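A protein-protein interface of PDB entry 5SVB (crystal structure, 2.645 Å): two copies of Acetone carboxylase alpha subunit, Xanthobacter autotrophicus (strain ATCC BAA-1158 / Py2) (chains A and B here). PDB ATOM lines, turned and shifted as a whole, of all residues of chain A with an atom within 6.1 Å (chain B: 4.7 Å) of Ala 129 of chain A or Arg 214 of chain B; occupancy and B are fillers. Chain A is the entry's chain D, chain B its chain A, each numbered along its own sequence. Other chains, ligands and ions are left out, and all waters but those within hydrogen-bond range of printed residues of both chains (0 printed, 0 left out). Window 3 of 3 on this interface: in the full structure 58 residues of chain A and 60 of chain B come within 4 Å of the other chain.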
ATOM      1  N   ASN A 125     -23.776 -13.382  23.334  1.00  0.00           N
ATOM      2  CA  ASN A 125     -22.964 -14.345  22.601  1.00  0.00           C
ATOM      3  C   ASN A 125     -23.492 -15.768  22.748  1.00  0.00           C
ATOM      4  O   ASN A 125     -22.745 -16.729  22.544  1.00  0.00           O
ATOM      5  CB  ASN A 125     -21.508 -14.252  23.057  1.00  0.00           C
ATOM      6  CG  ASN A 125     -20.881 -12.914  22.715  1.00  0.00           C
ATOM      7  OD1 ASN A 125     -20.232 -12.763  21.682  1.00  0.00           O
ATOM      8  ND2 ASN A 125     -21.082 -11.932  23.580  1.00  0.00           N
ATOM      9  N   ASN A 126     -24.766 -15.914  23.103  1.00  0.00           N
ATOM     10  CA  ASN A 126     -25.454 -17.201  23.083  1.00  0.00           C
ATOM     11  C   ASN A 126     -24.698 -18.255  23.890  1.00  0.00           C
ATOM     12  O   ASN A 126     -24.504 -19.391  23.453  1.00  0.00           O
ATOM     13  CB  ASN A 126     -25.675 -17.669  21.645  1.00  0.00           C
ATOM     14  CG  ASN A 126     -26.729 -18.753  21.537  1.00  0.00           C
ATOM     15  OD1 ASN A 126     -27.556 -18.926  22.432  1.00  0.00           O
ATOM     16  ND2 ASN A 126     -26.707 -19.487  20.435  1.00  0.00           N
ATOM     17  N   TRP A 127     -24.265 -17.864  25.091  1.00  0.00           N
ATOM     18  CA  TRP A 127     -23.783 -18.847  26.055  1.00  0.00           C
ATOM     19  C   TRP A 127     -24.841 -19.904  26.334  1.00  0.00           C
ATOM     20  O   TRP A 127     -24.509 -21.056  26.639  1.00  0.00           O
ATOM     21  CB  TRP A 127     -23.385 -18.155  27.357  1.00  0.00           C
ATOM     22  CG  TRP A 127     -21.912 -18.107  27.613  1.00  0.00           C
ATOM     23  CD1 TRP A 127     -21.264 -18.537  28.732  1.00  0.00           C
ATOM     24  CD2 TRP A 127     -20.902 -17.597  26.736  1.00  0.00           C
ATOM     25  NE1 TRP A 127     -19.914 -18.326  28.609  1.00  0.00           N
ATOM     26  CE2 TRP A 127     -19.664 -17.750  27.391  1.00  0.00           C
ATOM     27  CE3 TRP A 127     -20.924 -17.026  25.461  1.00  0.00           C
ATOM     28  CZ2 TRP A 127     -18.461 -17.355  26.814  1.00  0.00           C
ATOM     29  CZ3 TRP A 127     -19.727 -16.634  24.891  1.00  0.00           C
ATOM     30  CH2 TRP A 127     -18.512 -16.801  25.567  1.00  0.00           C
ATOM     31  N   GLU A 128     -26.117 -19.525  26.237  1.00  0.00           N
ATOM     32  CA  GLU A 128     -27.210 -20.458  26.490  1.00  0.00           C
ATOM     33  C   GLU A 128     -27.074 -21.719  25.646  1.00  0.00           C
ATOM     34  O   GLU A 128     -27.371 -22.825  26.114  1.00  0.00           O
ATOM     35  CB  GLU A 128     -28.542 -19.761  26.208  1.00  0.00           C
ATOM     36  CG  GLU A 128     -29.775 -20.557  26.584  1.00  0.00           C
ATOM     37  CD  GLU A 128     -31.044 -19.732  26.480  1.00  0.00           C
ATOM     38  OE1 GLU A 128     -30.937 -18.495  26.345  1.00  0.00           O
ATOM     39  OE2 GLU A 128     -32.146 -20.318  26.533  1.00  0.00           O
ATOM     40  N   ALA A 129     -26.628 -21.575  24.398  1.00  0.00           N
ATOM     41  CA  ALA A 129     -26.459 -22.718  23.510  1.00  0.00           C
ATOM     42  C   ALA A 129     -25.115 -23.407  23.689  1.00  0.00           C
ATOM     43  O   ALA A 129     -25.034 -24.632  23.555  1.00  0.00           O
ATOM     44  CB  ALA A 129     -26.609 -22.274  22.054  1.00  0.00           C
ATOM     45  N   ASN A 130     -24.066 -22.650  23.991  1.00  0.00           N
ATOM     46  CA  ASN A 130     -22.733 -23.205  24.173  1.00  0.00           C
ATOM     47  C   ASN A 130     -21.885 -22.192  24.942  1.00  0.00           C
ATOM     48  O   ASN A 130     -21.758 -21.048  24.511  1.00  0.00           O
ATOM     49  CB  ASN A 130     -22.098 -23.531  22.819  1.00  0.00           C
ATOM     50  CG  ASN A 130     -20.779 -24.277  22.947  1.00  0.00           C
ATOM     51  OD1 ASN A 130     -20.048 -24.116  23.923  1.00  0.00           O
ATOM     52  ND2 ASN A 130     -20.468 -25.095  21.950  1.00  0.00           N
ATOM     53  N   PRO A 131     -21.294 -22.598  26.080  1.00  0.00           N
ATOM     54  CA  PRO A 131     -21.273 -23.926  26.704  1.00  0.00           C
ATOM     55  C   PRO A 131     -22.533 -24.258  27.494  1.00  0.00           C
ATOM     56  O   PRO A 131     -22.584 -25.300  28.145  1.00  0.00           O
ATOM     57  CB  PRO A 131     -20.068 -23.838  27.636  1.00  0.00           C
ATOM     58  CG  PRO A 131     -20.055 -22.424  28.061  1.00  0.00           C
ATOM     59  CD  PRO A 131     -20.523 -21.623  26.874  1.00  0.00           C
ATOM     60  N   GLY A 132     -23.525 -23.385  27.448  1.00  0.00           N
ATOM     61  CA  GLY A 132     -24.757 -23.637  28.175  1.00  0.00           C
ATOM     62  C   GLY A 132     -24.730 -23.065  29.576  1.00  0.00           C
ATOM     63  O   GLY A 132     -23.690 -22.975  30.229  1.00  0.00           O
ATOM     64  N   VAL A 133     -25.909 -22.671  30.047  1.00  0.00           N
ATOM     65  CA  VAL A 133     -26.085 -22.080  31.367  1.00  0.00           C
ATOM     66  C   VAL A 133     -27.052 -22.977  32.126  1.00  0.00           C
ATOM     67  O   VAL A 133     -28.259 -22.968  31.857  1.00  0.00           O
ATOM     68  CB  VAL A 133     -26.607 -20.640  31.286  1.00  0.00           C
ATOM     69  CG1 VAL A 133     -26.710 -20.028  32.669  1.00  0.00           C
ATOM     70  CG2 VAL A 133     -25.703 -19.795  30.394  1.00  0.00           C
ATOM     71  N   LEU B 212     -15.987 -28.103  20.212  1.00  0.00           N
ATOM     72  CA  LEU B 212     -15.278 -27.148  21.047  1.00  0.00           C
ATOM     73  C   LEU B 212     -16.257 -26.282  21.832  1.00  0.00           C
ATOM     74  O   LEU B 212     -17.376 -26.007  21.389  1.00  0.00           O
ATOM     75  CB  LEU B 212     -14.371 -26.265  20.190  1.00  0.00           C
ATOM     76  CG  LEU B 212     -13.268 -27.011  19.437  1.00  0.00           C
ATOM     77  CD1 LEU B 212     -12.574 -26.089  18.460  1.00  0.00           C
ATOM     78  CD2 LEU B 212     -12.263 -27.607  20.407  1.00  0.00           C
ATOM     79  N   PHE B 213     -15.820 -25.854  23.012  1.00  0.00           N
ATOM     80  CA  PHE B 213     -16.645 -25.019  23.871  1.00  0.00           C
ATOM     81  C   PHE B 213     -16.523 -23.557  23.462  1.00  0.00           C
ATOM     82  O   PHE B 213     -15.432 -23.072  23.149  1.00  0.00           O
ATOM     83  CB  PHE B 213     -16.234 -25.194  25.333  1.00  0.00           C
ATOM     84  CG  PHE B 213     -16.339 -26.608  25.829  1.00  0.00           C
ATOM     85  CD1 PHE B 213     -17.425 -27.398  25.492  1.00  0.00           C
ATOM     86  CD2 PHE B 213     -15.350 -27.149  26.629  1.00  0.00           C
ATOM     87  CE1 PHE B 213     -17.522 -28.698  25.947  1.00  0.00           C
ATOM     88  CE2 PHE B 213     -15.442 -28.449  27.085  1.00  0.00           C
ATOM     89  CZ  PHE B 213     -16.529 -29.223  26.743  1.00  0.00           C
ATOM     90  N   ARG B 214     -17.655 -22.852  23.475  1.00  0.00           N
ATOM     91  CA  ARG B 214     -17.664 -21.467  23.015  1.00  0.00           C
ATOM     92  C   ARG B 214     -16.778 -20.586  23.886  1.00  0.00           C
ATOM     93  O   ARG B 214     -16.022 -19.753  23.372  1.00  0.00           O
ATOM     94  CB  ARG B 214     -19.092 -20.928  22.994  1.00  0.00           C
ATOM     95  CG  ARG B 214     -19.245 -19.671  22.162  1.00  0.00           C
ATOM     96  CD  ARG B 214     -20.560 -18.968  22.428  1.00  0.00           C
ATOM     97  NE  ARG B 214     -21.715 -19.790  22.085  1.00  0.00           N
ATOM     98  CZ  ARG B 214     -22.139 -20.004  20.844  1.00  0.00           C
ATOM     99  NH1 ARG B 214     -23.207 -20.761  20.630  1.00  0.00           N
ATOM    100  NH2 ARG B 214     -21.495 -19.472  19.816  1.00  0.00           N
ATOM    101  N   ASP B 215     -16.861 -20.744  25.209  1.00  0.00           N
ATOM    102  CA  ASP B 215     -16.042 -19.924  26.095  1.00  0.00           C
ATOM    103  C   ASP B 215     -14.558 -20.109  25.811  1.00  0.00           C
ATOM    104  O   ASP B 215     -13.764 -19.190  26.035  1.00  0.00           O
ATOM    105  CB  ASP B 215     -16.355 -20.248  27.557  1.00  0.00           C
ATOM    106  CG  ASP B 215     -16.147 -21.709  27.890  1.00  0.00           C
ATOM    107  OD1 ASP B 215     -16.363 -22.557  27.003  1.00  0.00           O
ATOM    108  OD2 ASP B 215     -15.773 -22.012  29.040  1.00  0.00           O
ATOM    109  N   TRP B 216     -14.164 -21.283  25.313  1.00  0.00           N
ATOM    110  CA  TRP B 216     -12.769 -21.499  24.943  1.00  0.00           C
ATOM    111  C   TRP B 216     -12.426 -20.789  23.637  1.00  0.00           C
ATOM    112  O   TRP B 216     -11.341 -20.212  23.507  1.00  0.00           O
ATOM    113  CB  TRP B 216     -12.485 -22.994  24.830  1.00  0.00           C
ATOM    114  CG  TRP B 216     -11.333 -23.322  23.932  1.00  0.00           C
ATOM    115  CD1 TRP B 216     -11.397 -23.884  22.693  1.00  0.00           C
ATOM    116  CD2 TRP B 216      -9.942 -23.104  24.200  1.00  0.00           C
ATOM    117  NE1 TRP B 216     -10.136 -24.036  22.175  1.00  0.00           N
ATOM    118  CE2 TRP B 216      -9.224 -23.561  23.079  1.00  0.00           C
ATOM    119  CE3 TRP B 216      -9.234 -22.565  25.277  1.00  0.00           C
ATOM    120  CZ2 TRP B 216      -7.839 -23.498  23.005  1.00  0.00           C
ATOM    121  CZ3 TRP B 216      -7.855 -22.503  25.201  1.00  0.00           C
ATOM    122  CH2 TRP B 216      -7.174 -22.967  24.073  1.00  0.00           C
ATOM    123  N   LEU B 217     -13.333 -20.819  22.661  1.00  0.00           N
ATOM    124  CA  LEU B 217     -13.068 -20.161  21.385  1.00  0.00           C
ATOM    125  C   LEU B 217     -12.957 -18.652  21.557  1.00  0.00           C
ATOM    126  O   LEU B 217     -12.033 -18.022  21.034  1.00  0.00           O
ATOM    127  CB  LEU B 217     -14.167 -20.512  20.383  1.00  0.00           C
ATOM    128  CG  LEU B 217     -14.232 -21.983  19.979  1.00  0.00           C
ATOM    129  CD1 LEU B 217     -15.503 -22.266  19.202  1.00  0.00           C
ATOM    130  CD2 LEU B 217     -13.009 -22.368  19.162  1.00  0.00           C
ATOM    131  N   HIS B 218     -13.900 -18.053  22.285  1.00  0.00           N
ATOM    132  CA  HIS B 218     -13.834 -16.618  22.541  1.00  0.00           C
ATOM    133  C   HIS B 218     -12.579 -16.257  23.321  1.00  0.00           C
ATOM    134  O   HIS B 218     -11.884 -15.292  22.987  1.00  0.00           O
ATOM    135  CB  HIS B 218     -15.081 -16.166  23.298  1.00  0.00           C
ATOM    136  CG  HIS B 218     -16.313 -16.102  22.450  1.00  0.00           C
ATOM    137  ND1 HIS B 218     -17.110 -14.982  22.381  1.00  0.00           N
ATOM    138  CD2 HIS B 218     -16.881 -17.018  21.632  1.00  0.00           C
ATOM    139  CE1 HIS B 218     -18.118 -15.211  21.560  1.00  0.00           C
ATOM    140  NE2 HIS B 218     -18.003 -16.440  21.092  1.00  0.00           N
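Of the 7 printed residues of chain B, 5 touch a printed residue of chain A.
Hydrophobic or aromatic side chains of chain B within 4 Å of the printed part of chain A: His 218.
Of the 9 printed residues of chain A, 6 touch a printed residue of chain B.
Printed residues of chain A that touch a printed residue of chain B: Asn 125, Asn 126, Trp 127, Ala 129, Asn 130 and Pro 131.
Hydrophobic or aromatic side chains of chain A that line the printed part of chain B: Trp 127, Ala 129 and Pro 131.
Of the printed residues of chain B, Asn 125 of chain A touches Arg 214 (3.1 Å) and His 218 (3.2 Å).
Of the printed residues of chain B, Asn 126 of chain A touches Arg 214 (3.1 Å).
Of the printed residues of chain B, Ala 129 of chain A touches Arg 214.
Val 133 of chain A touches none of the printed residues of chain B.
Printed residues of chain A within 4 Å of Arg 214 of chain B: Asn 125 (3.1 Å), Asn 126 (3.1 Å), Trp 127 (3.5 Å), Ala 129 (3.99 Å) and Asn 130 (2.7 Å).
The nearest printed residue of chain B that does not touch Ala 129 of chain A is Leu 212 of chain B (8.1 Å).
The nearest printed residue of chain B that does not touch Trp 127 of chain A is Trp 216 of chain B (6.0 Å).
The backbone carbonyl oxygen (O) of Trp 127 of chain A is in hydrogen-bond range of the backbone NH (N) of Gly 132 of chain A (2.7 Å).
The side-chain amide oxygen of Asn 126 of chain A sits at hydrogen-bond distance from the backbone NH of Ala 129 of chain A (3.4 Å).
No position is printed for both chains.
O of Leu 212 of chain B sits at hydrogen-bond distance from ND2 of Asn 130 of chain A (3.3 Å).
The guanidinium group (NE) of Arg 214 of chain B lies within hydrogen-bond range of the backbone carbonyl oxygen (O) of Asn 130 of chain A.
The guanidinium group (NE) of Arg 214 of chain B lies within hydrogen-bond range of the backbone carbonyl oxygen (O) of Asn 126 of chain A, 3.1 Å away.
The backbone carbonyl oxygen (O) of Asn 125 of chain A sits close to the guanidinium group (NE) of Arg 214 of chain B (3.3 Å).
Among the printed residues, pairs that only touch across the chains: Asn 125 of chain A with His 218 of chain B, Trp 127 of chain A with Arg 214 of chain B, Trp 127 of chain A with Asp 215 of chain B, Trp 127 of chain A with His 218 of chain B, Ala 129 of chain A with Arg 214 of chain B, Asn 130 of chain A with Phe 213 of chain B and Pro 131 of chain A with Asp 215 of chain B.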
